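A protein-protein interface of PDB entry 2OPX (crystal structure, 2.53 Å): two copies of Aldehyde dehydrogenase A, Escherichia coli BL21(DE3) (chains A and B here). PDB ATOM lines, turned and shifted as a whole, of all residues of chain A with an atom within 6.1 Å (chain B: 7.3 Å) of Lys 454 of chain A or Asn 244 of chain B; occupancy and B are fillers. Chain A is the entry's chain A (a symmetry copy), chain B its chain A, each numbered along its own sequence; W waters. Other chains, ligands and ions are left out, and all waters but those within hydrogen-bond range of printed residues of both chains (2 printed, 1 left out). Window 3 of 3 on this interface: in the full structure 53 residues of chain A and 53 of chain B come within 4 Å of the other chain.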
ATOM      1  N   VAL A 231       7.061  11.798  17.166  1.00  0.00           N
ATOM      2  CA  VAL A 231       6.839  13.220  17.366  1.00  0.00           C
ATOM      3  C   VAL A 231       5.396  13.562  17.047  1.00  0.00           C
ATOM      4  O   VAL A 231       4.710  14.199  17.847  1.00  0.00           O
ATOM      5  CB  VAL A 231       7.763  14.060  16.459  1.00  0.00           C
ATOM      6  CG1 VAL A 231       7.506  15.548  16.671  1.00  0.00           C
ATOM      7  CG2 VAL A 231       9.212  13.726  16.763  1.00  0.00           C
ATOM      8  N   GLU A 235       2.480  15.083  19.338  1.00  0.00           N
ATOM      9  CA  GLU A 235       1.738  16.285  18.993  1.00  0.00           C
ATOM     10  C   GLU A 235       0.257  16.039  19.236  1.00  0.00           C
ATOM     11  O   GLU A 235      -0.439  16.877  19.806  1.00  0.00           O
ATOM     12  CB  GLU A 235       1.950  16.637  17.524  1.00  0.00           C
ATOM     13  CG  GLU A 235       3.374  17.005  17.172  1.00  0.00           C
ATOM     14  CD  GLU A 235       3.541  17.268  15.691  1.00  0.00           C
ATOM     15  OE1 GLU A 235       2.627  17.883  15.095  1.00  0.00           O
ATOM     16  OE2 GLU A 235       4.586  16.870  15.129  1.00  0.00           O
ATOM     17  N   GLU A 251       8.529  11.747  25.480  1.00  0.00           N
ATOM     18  CA  GLU A 251       9.818  11.231  25.028  1.00  0.00           C
ATOM     19  C   GLU A 251       9.500  10.895  23.570  1.00  0.00           C
ATOM     20  O   GLU A 251       8.876   9.871  23.288  1.00  0.00           O
ATOM     21  CB  GLU A 251      10.159   9.963  25.816  1.00  0.00           C
ATOM     22  CG  GLU A 251      11.626   9.801  26.197  1.00  0.00           C
ATOM     23  CD  GLU A 251      12.486   9.262  25.072  1.00  0.00           C
ATOM     24  OE1 GLU A 251      12.573   9.931  24.018  1.00  0.00           O
ATOM     25  OE2 GLU A 251      13.076   8.170  25.245  1.00  0.00           O
ATOM     26  N   LEU A 252       9.923  11.758  22.647  1.00  0.00           N
ATOM     27  CA  LEU A 252       9.594  11.564  21.238  1.00  0.00           C
ATOM     28  C   LEU A 252      10.701  11.207  20.248  1.00  0.00           C
ATOM     29  O   LEU A 252      10.558  11.441  19.043  1.00  0.00           O
ATOM     30  CB  LEU A 252       8.857  12.805  20.727  1.00  0.00           C
ATOM     31  CG  LEU A 252       7.695  13.290  21.594  1.00  0.00           C
ATOM     32  CD1 LEU A 252       7.094  14.542  20.985  1.00  0.00           C
ATOM     33  CD2 LEU A 252       6.653  12.195  21.716  1.00  0.00           C
ATOM     34  N   GLY A 253      11.800  10.646  20.733  1.00  0.00           N
ATOM     35  CA  GLY A 253      12.859  10.256  19.820  1.00  0.00           C
ATOM     36  C   GLY A 253      13.973  11.258  19.628  1.00  0.00           C
ATOM     37  O   GLY A 253      14.015  12.297  20.285  1.00  0.00           O
ATOM     38  N   ASP A 408      15.736  19.225  15.264  1.00  0.00           N
ATOM     39  CA  ASP A 408      14.541  19.455  16.067  1.00  0.00           C
ATOM     40  C   ASP A 408      14.598  18.530  17.274  1.00  0.00           C
ATOM     41  O   ASP A 408      13.825  18.680  18.220  1.00  0.00           O
ATOM     42  CB  ASP A 408      13.267  19.179  15.268  1.00  0.00           C
ATOM     43  CG  ASP A 408      12.889  20.334  14.363  1.00  0.00           C
ATOM     44  OD1 ASP A 408      12.900  21.491  14.840  1.00  0.00           O
ATOM     45  OD2 ASP A 408      12.569  20.089  13.179  1.00  0.00           O
ATOM     46  N   TYR A 409      15.517  17.570  17.226  1.00  0.00           N
ATOM     47  CA  TYR A 409      15.711  16.622  18.312  1.00  0.00           C
ATOM     48  C   TYR A 409      16.933  17.037  19.120  1.00  0.00           C
ATOM     49  O   TYR A 409      17.902  17.543  18.564  1.00  0.00           O
ATOM     50  CB  TYR A 409      15.939  15.211  17.771  1.00  0.00           C
ATOM     51  CG  TYR A 409      14.781  14.640  16.993  1.00  0.00           C
ATOM     52  CD1 TYR A 409      14.840  14.529  15.602  1.00  0.00           C
ATOM     53  CD2 TYR A 409      13.636  14.175  17.646  1.00  0.00           C
ATOM     54  CE1 TYR A 409      13.791  13.963  14.876  1.00  0.00           C
ATOM     55  CE2 TYR A 409      12.580  13.606  16.932  1.00  0.00           C
ATOM     56  CZ  TYR A 409      12.666  13.501  15.545  1.00  0.00           C
ATOM     57  OH  TYR A 409      11.642  12.917  14.828  1.00  0.00           O
ATOM     58  N   GLY A 410      16.889  16.808  20.426  1.00  0.00           N
ATOM     59  CA  GLY A 410      18.002  17.166  21.281  1.00  0.00           C
ATOM     60  C   GLY A 410      18.056  16.264  22.495  1.00  0.00           C
ATOM     61  O   GLY A 410      18.276  16.722  23.622  1.00  0.00           O
ATOM     62  N   GLY A 451      14.860  14.797  26.865  1.00  0.00           N
ATOM     63  CA  GLY A 451      15.277  15.423  25.625  1.00  0.00           C
ATOM     64  C   GLY A 451      14.863  16.858  25.392  1.00  0.00           C
ATOM     65  O   GLY A 451      13.767  17.282  25.763  1.00  0.00           O
ATOM     66  N   TRP A 452      15.762  17.612  24.768  1.00  0.00           N
ATOM     67  CA  TRP A 452      15.505  19.008  24.441  1.00  0.00           C
ATOM     68  C   TRP A 452      14.652  19.105  23.188  1.00  0.00           C
ATOM     69  O   TRP A 452      14.427  18.111  22.483  1.00  0.00           O
ATOM     70  CB  TRP A 452      16.812  19.751  24.186  1.00  0.00           C
ATOM     71  CG  TRP A 452      17.650  19.925  25.398  1.00  0.00           C
ATOM     72  CD1 TRP A 452      17.719  19.089  26.473  1.00  0.00           C
ATOM     73  CD2 TRP A 452      18.596  20.968  25.637  1.00  0.00           C
ATOM     74  NE1 TRP A 452      18.655  19.545  27.364  1.00  0.00           N
ATOM     75  CE2 TRP A 452      19.211  20.697  26.877  1.00  0.00           C
ATOM     76  CE3 TRP A 452      18.986  22.106  24.923  1.00  0.00           C
ATOM     77  CZ2 TRP A 452      20.198  21.522  27.421  1.00  0.00           C
ATOM     78  CZ3 TRP A 452      19.968  22.930  25.467  1.00  0.00           C
ATOM     79  CH2 TRP A 452      20.561  22.631  26.702  1.00  0.00           C
ATOM     80  N   ARG A 453      14.181  20.316  22.918  1.00  0.00           N
ATOM     81  CA  ARG A 453      13.367  20.574  21.750  1.00  0.00           C
ATOM     82  C   ARG A 453      12.254  19.550  21.554  1.00  0.00           C
ATOM     83  O   ARG A 453      11.604  19.141  22.512  1.00  0.00           O
ATOM     84  CB  ARG A 453      14.272  20.652  20.518  1.00  0.00           C
ATOM     85  CG  ARG A 453      14.978  21.996  20.391  1.00  0.00           C
ATOM     86  CD  ARG A 453      16.154  21.949  19.428  1.00  0.00           C
ATOM     87  NE  ARG A 453      17.401  21.713  20.146  1.00  0.00           N
ATOM     88  CZ  ARG A 453      18.238  20.723  19.874  1.00  0.00           C
ATOM     89  NH1 ARG A 453      17.960  19.879  18.898  1.00  0.00           N
ATOM     90  NH2 ARG A 453      19.348  20.579  20.575  1.00  0.00           N
ATOM     91  N   LYS A 454      12.040  19.135  20.311  1.00  0.00           N
ATOM     92  CA  LYS A 454      10.978  18.192  20.004  1.00  0.00           C
ATOM     93  C   LYS A 454      11.206  16.785  20.538  1.00  0.00           C
ATOM     94  O   LYS A 454      10.318  15.939  20.454  1.00  0.00           O
ATOM     95  CB  LYS A 454      10.734  18.148  18.490  1.00  0.00           C
ATOM     96  CG  LYS A 454      10.306  19.490  17.906  1.00  0.00           C
ATOM     97  CD  LYS A 454       9.656  19.337  16.533  1.00  0.00           C
ATOM     98  CE  LYS A 454       9.139  20.681  16.033  1.00  0.00           C
ATOM     99  NZ  LYS A 454       8.323  20.582  14.792  1.00  0.00           N
ATOM    100  N   SER A 455      12.386  16.530  21.088  1.00  0.00           N
ATOM    101  CA  SER A 455      12.669  15.210  21.630  1.00  0.00           C
ATOM    102  C   SER A 455      11.765  14.908  22.820  1.00  0.00           C
ATOM    103  O   SER A 455      11.655  13.760  23.251  1.00  0.00           O
ATOM    104  CB  SER A 455      14.137  15.100  22.046  1.00  0.00           C
ATOM    105  OG  SER A 455      14.965  14.888  20.917  1.00  0.00           O
ATOM    106  N   GLY A 456      11.120  15.936  23.359  1.00  0.00           N
ATOM    107  CA  GLY A 456      10.223  15.694  24.471  1.00  0.00           C
ATOM    108  C   GLY A 456      10.005  16.825  25.452  1.00  0.00           C
ATOM    109  O   GLY A 456      10.495  17.943  25.266  1.00  0.00           O
ATOM    110  N   ALA B 217       3.132  31.140  21.076  1.00  0.00           N
ATOM    111  CA  ALA B 217       2.977  29.783  21.576  1.00  0.00           C
ATOM    112  C   ALA B 217       3.227  28.763  20.475  1.00  0.00           C
ATOM    113  O   ALA B 217       3.649  27.636  20.742  1.00  0.00           O
ATOM    114  CB  ALA B 217       1.572  29.591  22.149  1.00  0.00           C
ATOM    115  N   GLY B 218       2.973  29.170  19.236  1.00  0.00           N
ATOM    116  CA  GLY B 218       3.143  28.263  18.120  1.00  0.00           C
ATOM    117  C   GLY B 218       4.406  28.401  17.301  1.00  0.00           C
ATOM    118  O   GLY B 218       4.664  27.573  16.431  1.00  0.00           O
ATOM    119  N   ASN B 219       5.198  29.435  17.546  1.00  0.00           N
ATOM    120  CA  ASN B 219       6.418  29.582  16.779  1.00  0.00           C
ATOM    121  C   ASN B 219       7.384  28.476  17.211  1.00  0.00           C
ATOM    122  O   ASN B 219       7.723  28.361  18.388  1.00  0.00           O
ATOM    123  CB  ASN B 219       7.041  30.949  17.013  1.00  0.00           C
ATOM    124  CG  ASN B 219       8.256  31.171  16.157  1.00  0.00           C
ATOM    125  OD1 ASN B 219       9.240  30.437  16.258  1.00  0.00           O
ATOM    126  ND2 ASN B 219       8.199  32.179  15.298  1.00  0.00           N
ATOM    127  N   PRO B 220       7.844  27.653  16.253  1.00  0.00           N
ATOM    128  CA  PRO B 220       8.767  26.536  16.497  1.00  0.00           C
ATOM    129  C   PRO B 220      10.106  26.906  17.121  1.00  0.00           C
ATOM    130  O   PRO B 220      10.836  26.036  17.582  1.00  0.00           O
ATOM    131  CB  PRO B 220       8.919  25.911  15.112  1.00  0.00           C
ATOM    132  CG  PRO B 220       8.828  27.101  14.212  1.00  0.00           C
ATOM    133  CD  PRO B 220       7.653  27.859  14.805  1.00  0.00           C
ATOM    134  N   LYS B 221      10.441  28.189  17.129  1.00  0.00           N
ATOM    135  CA  LYS B 221      11.703  28.606  17.727  1.00  0.00           C
ATOM    136  C   LYS B 221      11.560  28.814  19.231  1.00  0.00           C
ATOM    137  O   LYS B 221      12.553  28.986  19.937  1.00  0.00           O
ATOM    138  CB  LYS B 221      12.199  29.905  17.095  1.00  0.00           C
ATOM    139  CG  LYS B 221      12.584  29.792  15.643  1.00  0.00           C
ATOM    140  CD  LYS B 221      13.240  31.075  15.176  1.00  0.00           C
ATOM    141  CE  LYS B 221      13.703  30.957  13.736  1.00  0.00           C
ATOM    142  NZ  LYS B 221      14.508  32.138  13.353  1.00  0.00           N
ATOM    143  N   VAL B 222      10.325  28.797  19.720  1.00  0.00           N
ATOM    144  CA  VAL B 222      10.071  29.006  21.136  1.00  0.00           C
ATOM    145  C   VAL B 222      10.246  27.743  21.972  1.00  0.00           C
ATOM    146  O   VAL B 222       9.595  26.723  21.724  1.00  0.00           O
ATOM    147  CB  VAL B 222       8.652  29.568  21.356  1.00  0.00           C
ATOM    148  CG1 VAL B 222       8.391  29.770  22.845  1.00  0.00           C
ATOM    149  CG2 VAL B 222       8.501  30.884  20.602  1.00  0.00           C
ATOM    150  N   ALA B 223      11.128  27.827  22.964  1.00  0.00           N
ATOM    151  CA  ALA B 223      11.416  26.707  23.860  1.00  0.00           C
ATOM    152  C   ALA B 223      10.275  26.488  24.857  1.00  0.00           C
ATOM    153  O   ALA B 223       9.901  25.353  25.151  1.00  0.00           O
ATOM    154  CB  ALA B 223      12.721  26.965  24.605  1.00  0.00           C
ATOM    155  N   ALA B 239      -2.674  23.829  23.283  1.00  0.00           N
ATOM    156  CA  ALA B 239      -2.977  23.090  22.067  1.00  0.00           C
ATOM    157  C   ALA B 239      -2.033  23.540  20.953  1.00  0.00           C
ATOM    158  O   ALA B 239      -1.516  22.724  20.189  1.00  0.00           O
ATOM    159  CB  ALA B 239      -4.423  23.327  21.664  1.00  0.00           C
ATOM    160  N   THR B 240      -1.814  24.847  20.866  1.00  0.00           N
ATOM    161  CA  THR B 240      -0.938  25.398  19.848  1.00  0.00           C
ATOM    162  C   THR B 240       0.508  24.990  20.099  1.00  0.00           C
ATOM    163  O   THR B 240       1.202  24.531  19.184  1.00  0.00           O
ATOM    164  CB  THR B 240      -1.036  26.929  19.822  1.00  0.00           C
ATOM    165  OG1 THR B 240      -2.328  27.305  19.338  1.00  0.00           O
ATOM    166  CG2 THR B 240       0.046  27.525  18.926  1.00  0.00           C
ATOM    167  N   ALA B 241       0.955  25.156  21.340  1.00  0.00           N
ATOM    168  CA  ALA B 241       2.316  24.804  21.726  1.00  0.00           C
ATOM    169  C   ALA B 241       2.590  23.332  21.438  1.00  0.00           C
ATOM    170  O   ALA B 241       3.738  22.914  21.307  1.00  0.00           O
ATOM    171  CB  ALA B 241       2.522  25.088  23.211  1.00  0.00           C
ATOM    172  N   ALA B 242       1.523  22.553  21.340  1.00  0.00           N
ATOM    173  CA  ALA B 242       1.634  21.128  21.083  1.00  0.00           C
ATOM    174  C   ALA B 242       2.198  20.836  19.699  1.00  0.00           C
ATOM    175  O   ALA B 242       2.934  19.867  19.509  1.00  0.00           O
ATOM    176  CB  ALA B 242       0.264  20.472  21.239  1.00  0.00           C
ATOM    177  N   LYS B 243       1.852  21.680  18.735  1.00  0.00           N
ATOM    178  CA  LYS B 243       2.305  21.504  17.362  1.00  0.00           C
ATOM    179  C   LYS B 243       3.809  21.380  17.244  1.00  0.00           C
ATOM    180  O   LYS B 243       4.309  20.649  16.392  1.00  0.00           O
ATOM    181  CB  LYS B 243       1.796  22.656  16.498  1.00  0.00           C
ATOM    182  CG  LYS B 243       0.280  22.692  16.459  1.00  0.00           C
ATOM    183  CD  LYS B 243      -0.278  23.789  15.574  1.00  0.00           C
ATOM    184  CE  LYS B 243      -1.805  23.750  15.609  1.00  0.00           C
ATOM    185  NZ  LYS B 243      -2.408  24.796  14.741  1.00  0.00           N
ATOM    186  N   ASN B 244       4.531  22.080  18.109  1.00  0.00           N
ATOM    187  CA  ASN B 244       5.984  22.023  18.077  1.00  0.00           C
ATOM    188  C   ASN B 244       6.568  21.463  19.362  1.00  0.00           C
ATOM    189  O   ASN B 244       7.752  21.653  19.651  1.00  0.00           O
ATOM    190  CB  ASN B 244       6.558  23.409  17.800  1.00  0.00           C
ATOM    191  CG  ASN B 244       6.261  23.885  16.394  1.00  0.00           C
ATOM    192  OD1 ASN B 244       6.605  23.218  15.416  1.00  0.00           O
ATOM    193  ND2 ASN B 244       5.623  25.041  16.284  1.00  0.00           N
ATOM    194  N   ILE B 245       5.735  20.760  20.123  1.00  0.00           N
ATOM    195  CA  ILE B 245       6.179  20.167  21.375  1.00  0.00           C
ATOM    196  C   ILE B 245       6.858  21.255  22.211  1.00  0.00           C
ATOM    197  O   ILE B 245       7.913  21.041  22.807  1.00  0.00           O
ATOM    198  CB  ILE B 245       7.178  19.013  21.108  1.00  0.00           C
ATOM    199  CG1 ILE B 245       6.640  18.099  20.000  1.00  0.00           C
ATOM    200  CG2 ILE B 245       7.407  18.211  22.380  1.00  0.00           C
ATOM    201  CD1 ILE B 245       5.296  17.456  20.297  1.00  0.00           C
ATOM    202  N   THR B 246       6.253  22.437  22.224  1.00  0.00           N
ATOM    203  CA  THR B 246       6.781  23.553  23.001  1.00  0.00           C
ATOM    204  C   THR B 246       6.363  23.401  24.458  1.00  0.00           C
ATOM    205  O   THR B 246       5.205  23.109  24.754  1.00  0.00           O
ATOM    206  CB  THR B 246       6.234  24.887  22.502  1.00  0.00           C
ATOM    207  OG1 THR B 246       6.631  25.076  21.141  1.00  0.00           O
ATOM    208  CG2 THR B 246       6.754  26.030  23.359  1.00  0.00           C
ATOM    209  N   LYS B 247       7.302  23.602  25.367  1.00  0.00           N
ATOM    210  CA  LYS B 247       6.989  23.483  26.780  1.00  0.00           C
ATOM    211  C   LYS B 247       6.056  24.617  27.192  1.00  0.00           C
ATOM    212  O   LYS B 247       6.163  25.737  26.689  1.00  0.00           O
ATOM    213  CB  LYS B 247       8.267  23.541  27.622  1.00  0.00           C
ATOM    214  CG  LYS B 247       8.016  23.323  29.106  1.00  0.00           C
ATOM    215  CD  LYS B 247       9.262  23.550  29.942  1.00  0.00           C
ATOM    216  CE  LYS B 247       8.950  23.349  31.417  1.00  0.00           C
ATOM    217  NZ  LYS B 247      10.055  23.791  32.314  1.00  0.00           N
HETATM  218  O   HOH W   1       6.436  19.108  16.055  1.00  0.00           O
HETATM  219  O   HOH W   2       8.811  22.893  12.833  1.00  0.00           O
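The backbone carbonyl oxygen (O) of Gly 218 of chain B is in hydrogen-bond range of the side-chain amide nitrogen (ND2) of Asn 244 of chain B, 2.7 Å away. The backbone NH of Leu 252 of chain A sits at hydrogen-bond distance from the backbone carbonyl oxygen of Ser 455 of chain A (2.7 Å). The backbone NH (N) of Lys 454 of chain A is in hydrogen-bond range of the backbone carbonyl oxygen (O) of Asp 408 of chain A (2.8 Å).
Water W1 lies within hydrogen-bond range of the backbone carbonyl oxygen (O) of Lys 243 of chain B (2.6 Å), the side-chain amino group (NZ) of Lys 454 of chain A (2.7 Å) and the side-chain carboxylate (OE2) of Glu 235 of chain A (3.0 Å). Water W2 lies within hydrogen-bond range of NZ of Lys 454 of chain A (3.1 Å) and OD1 of Asn 244 of chain B (3.4 Å).
Glu 235 of chain A touches Ala 242 of chain B. Glu 235 of chain A touches Ile 245 of chain B (CG to CD1, 3.7 Å). Leu 252 of chain A touches Ile 245 of chain B.
No position is printed for both chains.
OD1 of Asn 244 of chain B is in hydrogen-bond range of NZ of Lys 454 of chain A, 3.2 Å away. The side-chain carboxylate (OE1) of Glu 235 of chain A sits close to the backbone carbonyl oxygen (O) of Lys 243 of chain B, 3.5 Å away.
Printed residues of chain B within 4 Å of Glu 235 of chain A: Ala 242 (3.7 Å), Lys 243 (3.5 Å) and Ile 245 (3.7 Å). Tyr 409 of chain A touches none of the printed residues of chain B. Printed residues of chain B within 4 Å of Lys 454 of chain A: Asn 244 (3.2 Å). Asn 219 of chain B touches none of the printed residues of chain A. Of the printed residues of chain A, Ile 245 of chain B touches Glu 235 (3.7 Å) and Leu 252 (3.5 Å). The nearest residue of chain A that does not touch Asn 244 of chain B is Glu 235 of chain A (5.3 Å).
Of the 14 printed residues of chain A, 3 touch a printed residue of chain B. Printed residues of chain A that touch a printed residue of chain B: Glu 235, Leu 252 and Lys 454. Hydrophobic or aromatic side chains of chain A that line the printed part of chain B: Leu 252. Among the printed residues, 5 pairs touch across the chains.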
